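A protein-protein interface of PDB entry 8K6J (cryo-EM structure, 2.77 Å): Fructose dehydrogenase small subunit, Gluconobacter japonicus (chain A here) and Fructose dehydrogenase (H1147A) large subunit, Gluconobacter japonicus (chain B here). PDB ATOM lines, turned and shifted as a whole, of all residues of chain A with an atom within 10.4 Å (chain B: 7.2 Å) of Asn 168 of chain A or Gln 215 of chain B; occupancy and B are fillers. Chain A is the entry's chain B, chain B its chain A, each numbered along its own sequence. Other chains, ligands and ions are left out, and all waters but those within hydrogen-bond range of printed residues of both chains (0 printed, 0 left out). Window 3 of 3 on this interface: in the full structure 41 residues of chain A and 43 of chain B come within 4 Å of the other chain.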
ATOM      1  N   ALA A 163      38.206   2.753  13.088  1.00  0.00           N
ATOM      2  CA  ALA A 163      37.275   1.933  12.330  1.00  0.00           C
ATOM      3  C   ALA A 163      37.516   0.446  12.556  1.00  0.00           C
ATOM      4  O   ALA A 163      38.642   0.000  12.790  1.00  0.00           O
ATOM      5  CB  ALA A 163      37.389   2.244  10.841  1.00  0.00           C
ATOM      6  N   HIS A 164      36.435  -0.322  12.478  1.00  0.00           N
ATOM      7  CA  HIS A 164      36.514  -1.772  12.389  1.00  0.00           C
ATOM      8  C   HIS A 164      36.806  -2.150  10.936  1.00  0.00           C
ATOM      9  O   HIS A 164      37.086  -1.294  10.094  1.00  0.00           O
ATOM     10  CB  HIS A 164      35.227  -2.402  12.910  1.00  0.00           C
ATOM     11  CG  HIS A 164      35.437  -3.423  13.982  1.00  0.00           C
ATOM     12  ND1 HIS A 164      34.894  -4.688  13.920  1.00  0.00           N
ATOM     13  CD2 HIS A 164      36.121  -3.365  15.148  1.00  0.00           C
ATOM     14  CE1 HIS A 164      35.240  -5.367  14.998  1.00  0.00           C
ATOM     15  NE2 HIS A 164      35.984  -4.587  15.760  1.00  0.00           N
ATOM     16  N   ASN A 165      36.721  -3.436  10.611  1.00  0.00           N
ATOM     17  CA  ASN A 165      37.153  -3.911   9.299  1.00  0.00           C
ATOM     18  C   ASN A 165      36.076  -3.626   8.263  1.00  0.00           C
ATOM     19  O   ASN A 165      35.118  -4.386   8.117  1.00  0.00           O
ATOM     20  CB  ASN A 165      37.482  -5.398   9.348  1.00  0.00           C
ATOM     21  CG  ASN A 165      36.409  -6.208  10.031  1.00  0.00           C
ATOM     22  OD1 ASN A 165      35.479  -5.657  10.612  1.00  0.00           O
ATOM     23  ND2 ASN A 165      36.528  -7.527   9.961  1.00  0.00           N
ATOM     24  N   GLY A 166      36.231  -2.528   7.528  1.00  0.00           N
ATOM     25  CA  GLY A 166      35.429  -2.287   6.352  1.00  0.00           C
ATOM     26  C   GLY A 166      34.143  -1.540   6.624  1.00  0.00           C
ATOM     27  O   GLY A 166      33.668  -1.458   7.759  1.00  0.00           O
ATOM     28  N   PRO A 167      33.547  -0.981   5.568  1.00  0.00           N
ATOM     29  CA  PRO A 167      32.350  -0.149   5.729  1.00  0.00           C
ATOM     30  C   PRO A 167      31.039  -0.910   5.822  1.00  0.00           C
ATOM     31  O   PRO A 167      29.983  -0.270   5.802  1.00  0.00           O
ATOM     32  CB  PRO A 167      32.372   0.729   4.466  1.00  0.00           C
ATOM     33  CG  PRO A 167      33.742   0.588   3.907  1.00  0.00           C
ATOM     34  CD  PRO A 167      34.151  -0.799   4.243  1.00  0.00           C
ATOM     35  N   ASN A 168      31.044  -2.239   5.883  1.00  0.00           N
ATOM     36  CA  ASN A 168      29.793  -2.956   6.097  1.00  0.00           C
ATOM     37  C   ASN A 168      29.986  -4.176   6.987  1.00  0.00           C
ATOM     38  O   ASN A 168      29.307  -5.192   6.806  1.00  0.00           O
ATOM     39  CB  ASN A 168      29.154  -3.365   4.772  1.00  0.00           C
ATOM     40  CG  ASN A 168      28.160  -2.339   4.267  1.00  0.00           C
ATOM     41  OD1 ASN A 168      27.577  -1.590   5.048  1.00  0.00           O
ATOM     42  ND2 ASN A 168      27.958  -2.302   2.957  1.00  0.00           N
ATOM     43  N   TYR A 169      30.905  -4.100   7.949  1.00  0.00           N
ATOM     44  CA  TYR A 169      31.207  -5.264   8.772  1.00  0.00           C
ATOM     45  C   TYR A 169      30.030  -5.673   9.646  1.00  0.00           C
ATOM     46  O   TYR A 169      29.914  -6.849  10.008  1.00  0.00           O
ATOM     47  CB  TYR A 169      32.432  -4.989   9.641  1.00  0.00           C
ATOM     48  CG  TYR A 169      32.206  -3.950  10.715  1.00  0.00           C
ATOM     49  CD1 TYR A 169      32.378  -2.602  10.446  1.00  0.00           C
ATOM     50  CD2 TYR A 169      31.829  -4.319  11.997  1.00  0.00           C
ATOM     51  CE1 TYR A 169      32.174  -1.653  11.420  1.00  0.00           C
ATOM     52  CE2 TYR A 169      31.622  -3.375  12.975  1.00  0.00           C
ATOM     53  CZ  TYR A 169      31.796  -2.044  12.681  1.00  0.00           C
ATOM     54  OH  TYR A 169      31.592  -1.097  13.655  1.00  0.00           O
ATOM     55  N   TRP A 170      29.149  -4.734   9.993  1.00  0.00           N
ATOM     56  CA  TRP A 170      28.101  -5.030  10.962  1.00  0.00           C
ATOM     57  C   TRP A 170      27.025  -5.957  10.416  1.00  0.00           C
ATOM     58  O   TRP A 170      26.173  -6.405  11.189  1.00  0.00           O
ATOM     59  CB  TRP A 170      27.459  -3.738  11.464  1.00  0.00           C
ATOM     60  CG  TRP A 170      27.038  -2.798  10.391  1.00  0.00           C
ATOM     61  CD1 TRP A 170      25.846  -2.787   9.735  1.00  0.00           C
ATOM     62  CD2 TRP A 170      27.801  -1.716   9.855  1.00  0.00           C
ATOM     63  NE1 TRP A 170      25.819  -1.767   8.820  1.00  0.00           N
ATOM     64  CE2 TRP A 170      27.010  -1.093   8.875  1.00  0.00           C
ATOM     65  CE3 TRP A 170      29.077  -1.214  10.107  1.00  0.00           C
ATOM     66  CZ2 TRP A 170      27.455   0.001   8.148  1.00  0.00           C
ATOM     67  CZ3 TRP A 170      29.515  -0.129   9.383  1.00  0.00           C
ATOM     68  CH2 TRP A 170      28.707   0.470   8.421  1.00  0.00           C
ATOM     69  N   VAL A 171      27.032  -6.246   9.114  1.00  0.00           N
ATOM     70  CA  VAL A 171      26.082  -7.208   8.566  1.00  0.00           C
ATOM     71  C   VAL A 171      26.314  -8.591   9.159  1.00  0.00           C
ATOM     72  O   VAL A 171      25.376  -9.385   9.292  1.00  0.00           O
ATOM     73  CB  VAL A 171      26.178  -7.226   7.030  1.00  0.00           C
ATOM     74  CG1 VAL A 171      25.043  -8.037   6.435  1.00  0.00           C
ATOM     75  CG2 VAL A 171      26.157  -5.813   6.490  1.00  0.00           C
ATOM     76  N   SER A 172      27.552  -8.899   9.529  1.00  0.00           N
ATOM     77  CA  SER A 172      27.874 -10.197  10.101  1.00  0.00           C
ATOM     78  C   SER A 172      27.353 -10.306  11.529  1.00  0.00           C
ATOM     79  O   SER A 172      27.204  -9.309  12.239  1.00  0.00           O
ATOM     80  CB  SER A 172      29.383 -10.427  10.081  1.00  0.00           C
ATOM     81  OG  SER A 172      30.021  -9.678  11.100  1.00  0.00           O
ATOM     82  N   GLU A 173      27.076 -11.539  11.943  1.00  0.00           N
ATOM     83  CA  GLU A 173      26.602 -11.783  13.294  1.00  0.00           C
ATOM     84  C   GLU A 173      27.723 -11.542  14.304  1.00  0.00           C
ATOM     85  O   GLU A 173      28.896 -11.787  14.015  1.00  0.00           O
ATOM     86  CB  GLU A 173      26.083 -13.211  13.427  1.00  0.00           C
ATOM     87  CG  GLU A 173      24.698 -13.468  12.827  1.00  0.00           C
ATOM     88  CD  GLU A 173      23.722 -12.318  13.019  1.00  0.00           C
ATOM     89  OE1 GLU A 173      22.857 -12.425  13.913  1.00  0.00           O
ATOM     90  OE2 GLU A 173      23.784 -11.331  12.255  1.00  0.00           O
ATOM     91  N   MET B 178      22.132   2.244   4.379  1.00  0.00           N
ATOM     92  CA  MET B 178      23.123   1.227   4.677  1.00  0.00           C
ATOM     93  C   MET B 178      22.505   0.128   5.541  1.00  0.00           C
ATOM     94  O   MET B 178      21.553   0.376   6.285  1.00  0.00           O
ATOM     95  CB  MET B 178      24.327   1.851   5.381  1.00  0.00           C
ATOM     96  CG  MET B 178      24.141   2.084   6.864  1.00  0.00           C
ATOM     97  SD  MET B 178      25.577   2.841   7.645  1.00  0.00           S
ATOM     98  CE  MET B 178      26.200   3.841   6.303  1.00  0.00           C
ATOM     99  N   PRO B 179      23.007  -1.101   5.436  1.00  0.00           N
ATOM    100  CA  PRO B 179      22.393  -2.211   6.174  1.00  0.00           C
ATOM    101  C   PRO B 179      22.484  -2.017   7.680  1.00  0.00           C
ATOM    102  O   PRO B 179      23.422  -1.410   8.199  1.00  0.00           O
ATOM    103  CB  PRO B 179      23.201  -3.432   5.717  1.00  0.00           C
ATOM    104  CG  PRO B 179      24.462  -2.875   5.155  1.00  0.00           C
ATOM    105  CD  PRO B 179      24.097  -1.559   4.562  1.00  0.00           C
ATOM    106  N   TYR B 180      21.485  -2.551   8.376  1.00  0.00           N
ATOM    107  CA  TYR B 180      21.395  -2.416   9.823  1.00  0.00           C
ATOM    108  C   TYR B 180      22.538  -3.144  10.519  1.00  0.00           C
ATOM    109  O   TYR B 180      23.060  -4.146  10.027  1.00  0.00           O
ATOM    110  CB  TYR B 180      20.073  -2.988  10.326  1.00  0.00           C
ATOM    111  CG  TYR B 180      18.905  -2.035  10.309  1.00  0.00           C
ATOM    112  CD1 TYR B 180      19.096  -0.664  10.282  1.00  0.00           C
ATOM    113  CD2 TYR B 180      17.605  -2.516  10.330  1.00  0.00           C
ATOM    114  CE1 TYR B 180      18.023   0.199  10.270  1.00  0.00           C
ATOM    115  CE2 TYR B 180      16.530  -1.663  10.318  1.00  0.00           C
ATOM    116  CZ  TYR B 180      16.744  -0.308  10.290  1.00  0.00           C
ATOM    117  OH  TYR B 180      15.663   0.537  10.279  1.00  0.00           O
ATOM    118  N   ARG B 205      24.441  10.552   5.295  1.00  0.00           N
ATOM    119  CA  ARG B 205      25.598   9.684   5.420  1.00  0.00           C
ATOM    120  C   ARG B 205      25.846   8.994   4.089  1.00  0.00           C
ATOM    121  O   ARG B 205      24.950   8.883   3.251  1.00  0.00           O
ATOM    122  CB  ARG B 205      25.394   8.641   6.523  1.00  0.00           C
ATOM    123  CG  ARG B 205      26.642   8.297   7.295  1.00  0.00           C
ATOM    124  CD  ARG B 205      26.298   7.634   8.611  1.00  0.00           C
ATOM    125  NE  ARG B 205      25.157   8.251   9.275  1.00  0.00           N
ATOM    126  CZ  ARG B 205      25.204   9.398   9.936  1.00  0.00           C
ATOM    127  NH1 ARG B 205      26.325  10.091  10.039  1.00  0.00           N
ATOM    128  NH2 ARG B 205      24.101   9.858  10.514  1.00  0.00           N
ATOM    129  N   ASN B 206      27.073   8.524   3.903  1.00  0.00           N
ATOM    130  CA  ASN B 206      27.487   7.903   2.648  1.00  0.00           C
ATOM    131  C   ASN B 206      27.434   6.388   2.801  1.00  0.00           C
ATOM    132  O   ASN B 206      28.315   5.784   3.417  1.00  0.00           O
ATOM    133  CB  ASN B 206      28.884   8.367   2.256  1.00  0.00           C
ATOM    134  CG  ASN B 206      28.931   9.834   1.912  1.00  0.00           C
ATOM    135  OD1 ASN B 206      27.911  10.520   1.931  1.00  0.00           O
ATOM    136  ND2 ASN B 206      30.117  10.329   1.595  1.00  0.00           N
ATOM    137  N   SER B 207      26.396   5.772   2.235  1.00  0.00           N
ATOM    138  CA  SER B 207      26.388   4.326   2.064  1.00  0.00           C
ATOM    139  C   SER B 207      27.258   3.890   0.897  1.00  0.00           C
ATOM    140  O   SER B 207      27.469   2.688   0.710  1.00  0.00           O
ATOM    141  CB  SER B 207      24.962   3.820   1.857  1.00  0.00           C
ATOM    142  OG  SER B 207      24.506   4.114   0.551  1.00  0.00           O
ATOM    143  N   ARG B 208      27.743   4.841   0.111  1.00  0.00           N
ATOM    144  CA  ARG B 208      28.692   4.620  -0.968  1.00  0.00           C
ATOM    145  C   ARG B 208      29.470   5.910  -1.151  1.00  0.00           C
ATOM    146  O   ARG B 208      29.016   6.973  -0.713  1.00  0.00           O
ATOM    147  CB  ARG B 208      27.979   4.221  -2.265  1.00  0.00           C
ATOM    148  CG  ARG B 208      27.059   5.294  -2.803  1.00  0.00           C
ATOM    149  CD  ARG B 208      26.377   4.850  -4.080  1.00  0.00           C
ATOM    150  NE  ARG B 208      25.402   5.830  -4.537  1.00  0.00           N
ATOM    151  CZ  ARG B 208      25.713   6.961  -5.154  1.00  0.00           C
ATOM    152  NH1 ARG B 208      26.970   7.287  -5.408  1.00  0.00           N
ATOM    153  NH2 ARG B 208      24.739   7.786  -5.526  1.00  0.00           N
ATOM    154  N   PRO B 209      30.652   5.853  -1.760  1.00  0.00           N
ATOM    155  CA  PRO B 209      31.415   7.087  -1.977  1.00  0.00           C
ATOM    156  C   PRO B 209      30.587   8.113  -2.731  1.00  0.00           C
ATOM    157  O   PRO B 209      29.890   7.793  -3.695  1.00  0.00           O
ATOM    158  CB  PRO B 209      32.617   6.615  -2.796  1.00  0.00           C
ATOM    159  CG  PRO B 209      32.806   5.214  -2.373  1.00  0.00           C
ATOM    160  CD  PRO B 209      31.435   4.659  -2.119  1.00  0.00           C
ATOM    161  N   TYR B 210      30.668   9.362  -2.280  1.00  0.00           N
ATOM    162  CA  TYR B 210      29.760  10.394  -2.757  1.00  0.00           C
ATOM    163  C   TYR B 210      30.391  11.754  -2.522  1.00  0.00           C
ATOM    164  O   TYR B 210      30.957  11.994  -1.452  1.00  0.00           O
ATOM    165  CB  TYR B 210      28.423  10.294  -2.028  1.00  0.00           C
ATOM    166  CG  TYR B 210      27.316  11.176  -2.553  1.00  0.00           C
ATOM    167  CD1 TYR B 210      27.174  12.481  -2.113  1.00  0.00           C
ATOM    168  CD2 TYR B 210      26.382  10.685  -3.454  1.00  0.00           C
ATOM    169  CE1 TYR B 210      26.154  13.282  -2.577  1.00  0.00           C
ATOM    170  CE2 TYR B 210      25.358  11.478  -3.920  1.00  0.00           C
ATOM    171  CZ  TYR B 210      25.248  12.774  -3.479  1.00  0.00           C
ATOM    172  OH  TYR B 210      24.228  13.565  -3.947  1.00  0.00           O
ATOM    173  N   ARG B 213      33.635  12.074  -0.880  1.00  0.00           N
ATOM    174  CA  ARG B 213      33.763  11.698   0.514  1.00  0.00           C
ATOM    175  C   ARG B 213      33.558  10.198   0.675  1.00  0.00           C
ATOM    176  O   ARG B 213      32.747   9.605  -0.044  1.00  0.00           O
ATOM    177  CB  ARG B 213      32.751  12.447   1.384  1.00  0.00           C
ATOM    178  CG  ARG B 213      32.986  13.939   1.451  1.00  0.00           C
ATOM    179  CD  ARG B 213      31.975  14.594   2.356  1.00  0.00           C
ATOM    180  NE  ARG B 213      30.761  14.958   1.640  1.00  0.00           N
ATOM    181  CZ  ARG B 213      29.609  14.311   1.742  1.00  0.00           C
ATOM    182  NH1 ARG B 213      29.481  13.249   2.518  1.00  0.00           N
ATOM    183  NH2 ARG B 213      28.561  14.738   1.046  1.00  0.00           N
ATOM    184  N   PRO B 214      34.272   9.560   1.595  1.00  0.00           N
ATOM    185  CA  PRO B 214      34.257   8.097   1.655  1.00  0.00           C
ATOM    186  C   PRO B 214      32.954   7.550   2.211  1.00  0.00           C
ATOM    187  O   PRO B 214      32.135   8.263   2.791  1.00  0.00           O
ATOM    188  CB  PRO B 214      35.427   7.772   2.588  1.00  0.00           C
ATOM    189  CG  PRO B 214      35.557   8.974   3.441  1.00  0.00           C
ATOM    190  CD  PRO B 214      35.199  10.141   2.578  1.00  0.00           C
ATOM    191  N   GLN B 215      32.779   6.247   2.019  1.00  0.00           N
ATOM    192  CA  GLN B 215      31.688   5.520   2.644  1.00  0.00           C
ATOM    193  C   GLN B 215      31.959   5.366   4.135  1.00  0.00           C
ATOM    194  O   GLN B 215      33.101   5.166   4.557  1.00  0.00           O
ATOM    195  CB  GLN B 215      31.540   4.148   1.987  1.00  0.00           C
ATOM    196  CG  GLN B 215      30.386   3.313   2.484  1.00  0.00           C
ATOM    197  CD  GLN B 215      30.262   2.008   1.729  1.00  0.00           C
ATOM    198  OE1 GLN B 215      30.885   1.820   0.688  1.00  0.00           O
ATOM    199  NE2 GLN B 215      29.459   1.094   2.256  1.00  0.00           N
ATOM    200  N   CYS B 216      30.905   5.465   4.944  1.00  0.00           N
ATOM    201  CA  CYS B 216      31.093   5.378   6.386  1.00  0.00           C
ATOM    202  C   CYS B 216      31.510   3.972   6.782  1.00  0.00           C
ATOM    203  O   CYS B 216      30.822   2.996   6.477  1.00  0.00           O
ATOM    204  CB  CYS B 216      29.826   5.775   7.143  1.00  0.00           C
ATOM    205  SG  CYS B 216      30.136   6.093   8.923  1.00  0.00           S
ATOM    206  N   CYS B 217      32.635   3.879   7.481  1.00  0.00           N
ATOM    207  CA  CYS B 217      33.138   2.620   8.000  1.00  0.00           C
ATOM    208  C   CYS B 217      32.492   2.239   9.319  1.00  0.00           C
ATOM    209  O   CYS B 217      32.983   1.330   9.996  1.00  0.00           O
ATOM    210  CB  CYS B 217      34.655   2.691   8.167  1.00  0.00           C
ATOM    211  SG  CYS B 217      35.237   4.231   8.891  1.00  0.00           S
ATOM    212  N   GLY B 218      31.408   2.904   9.696  1.00  0.00           N
ATOM    213  CA  GLY B 218      30.770   2.627  10.967  1.00  0.00           C
ATOM    214  C   GLY B 218      31.618   2.966  12.171  1.00  0.00           C
ATOM    215  O   GLY B 218      31.730   2.148  13.093  1.00  0.00           O
ATOM    216  N   ASN B 219      32.233   4.149  12.182  1.00  0.00           N
ATOM    217  CA  ASN B 219      32.943   4.589  13.373  1.00  0.00           C
ATOM    218  C   ASN B 219      32.010   4.789  14.557  1.00  0.00           C
ATOM    219  O   ASN B 219      32.478   4.848  15.694  1.00  0.00           O
ATOM    220  CB  ASN B 219      33.711   5.883  13.099  1.00  0.00           C
ATOM    221  CG  ASN B 219      34.780   5.714  12.047  1.00  0.00           C
ATOM    222  OD1 ASN B 219      35.540   4.751  12.071  1.00  0.00           O
ATOM    223  ND2 ASN B 219      34.850   6.654  11.118  1.00  0.00           N
ATOM    224  N   ILE B 228      36.446  10.412   9.350  1.00  0.00           N
ATOM    225  CA  ILE B 228      36.720  10.318   7.925  1.00  0.00           C
ATOM    226  C   ILE B 228      35.838  11.233   7.102  1.00  0.00           C
ATOM    227  O   ILE B 228      35.996  11.288   5.876  1.00  0.00           O
ATOM    228  CB  ILE B 228      36.590   8.866   7.435  1.00  0.00           C
ATOM    229  CG1 ILE B 228      35.124   8.494   7.260  1.00  0.00           C
ATOM    230  CG2 ILE B 228      37.203   7.937   8.443  1.00  0.00           C
ATOM    231  CD1 ILE B 228      34.925   7.140   6.635  1.00  0.00           C
ATOM    232  N   GLY B 229      34.921  11.959   7.731  1.00  0.00           N
ATOM    233  CA  GLY B 229      34.050  12.859   6.997  1.00  0.00           C
ATOM    234  C   GLY B 229      33.057  12.169   6.089  1.00  0.00           C
ATOM    235  O   GLY B 229      32.821  12.637   4.969  1.00  0.00           O
ATOM    236  N   ALA B 230      32.465  11.067   6.542  1.00  0.00           N
ATOM    237  CA  ALA B 230      31.491  10.355   5.731  1.00  0.00           C
ATOM    238  C   ALA B 230      30.065  10.842   5.939  1.00  0.00           C
ATOM    239  O   ALA B 230      29.156  10.334   5.276  1.00  0.00           O
ATOM    240  CB  ALA B 230      31.563   8.859   6.021  1.00  0.00           C
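SG of Cys 217 of chain B touches CB of Ala 163 of chain A (3.5 Å). Cys 217 of chain B touches Gly 166 of chain A. Pro 167 of chain A touches Gln 215 of chain B. CA of Pro 167 of chain A touches CA of Cys 217 of chain B, 3.7 Å away. Tyr 169 of chain A touches Cys 217 of chain B (CE1 to O, 3.4 Å). Trp 170 of chain A touches Met 178 of chain B (CZ2 to SD, 3.4 Å). O of Tyr 180 of chain B touches CD1 of Trp 170 of chain A, at 3.1 Å. Cys 216 of chain B touches Trp 170 of chain A. Trp 170 of chain A touches Cys 217 of chain B. CG2 of Val 171 of chain A touches CG of Pro 179 of chain B, 3.6 Å away.
O of Pro 179 of chain B lies within hydrogen-bond range of NE1 of Trp 170 of chain A. The side-chain hydroxyl (OH) of Tyr 169 of chain A sits at hydrogen-bond distance from the backbone carbonyl oxygen (O) of Gly 218 of chain B, at 3.3 Å. The side-chain amide oxygen (OD1) of Asn 219 of chain B lies close to the backbone NH (N) of Ala 163 of chain A, at 3.5 Å. The backbone carbonyl oxygen (O) of Cys 216 of chain B sits close to the backbone carbonyl oxygen (O) of Pro 167 of chain A, at 3.4 Å.
The backbone carbonyl oxygen of Asn 206 of chain B is in hydrogen-bond range of the backbone NH of Cys 216 of chain B. O of Ser 207 of chain B sits at hydrogen-bond distance from NE2 of Gln 215 of chain B (3.0 Å). N of Gly 218 of chain B sits close to SG of Cys 216 of chain B, 3.5 Å away. The side-chain amide oxygen of Asn 219 of chain B lies within hydrogen-bond range of the side-chain sulfur of Cys 217 of chain B (3.2 Å). The side-chain hydroxyl of Ser 172 of chain A lies within hydrogen-bond range of the backbone carbonyl oxygen of Tyr 169 of chain A, at 3.0 Å.
Of the 11 printed residues of chain A, 7 touch a printed residue of chain B. Hydrophobic or aromatic side chains of chain A that line the printed part of chain B: Ala 163, Pro 167, Tyr 169, Trp 170 and Val 171. Along chain A the printed residues that touch a printed residue of chain B span positions 163 to 171.
Asn 168 of chain A touches just these residues of chain B: Pro 179 and Gln 215. Gln 215 of chain B touches just these residues of chain A: Pro 167 (3.7 Å) and Asn 168 (3.8 Å). No residue of chain A comes within 4 Å of Asn 206 of chain B. No residue of chain A comes within 4 Å of Pro 214 of chain B. Of chain A, only Pro 167 and Trp 170 come within 4 Å of Cys 216 of chain B. Of chain A, only Ala 163, Gly 166, Pro 167, Tyr 169 and Trp 170 come within 4 Å of Cys 217 of chain B. No residue of chain A comes within 4 Å of Ala 230 of chain B. Printed residues of chain A within 4 Å of Met 178 of chain B: Trp 170 (3.4 Å). Printed residues of chain B within 4 Å of Ala 163 of chain A: Cys 217 and Asn 219. Of the printed residues of chain A, Tyr 180 of chain B touches Trp 170. Printed residues of chain B within 4 Å of Tyr 169 of chain A: Cys 217 (3.4 Å) and Gly 218 (3.3 Å). The nearest residue of chain A that does not touch Gln 215 of chain B is Trp 170 of chain A (6.2 Å). The nearest printed residue of chain B that does not touch Tyr 169 of chain A is Asn 219 of chain B (5.5 Å).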
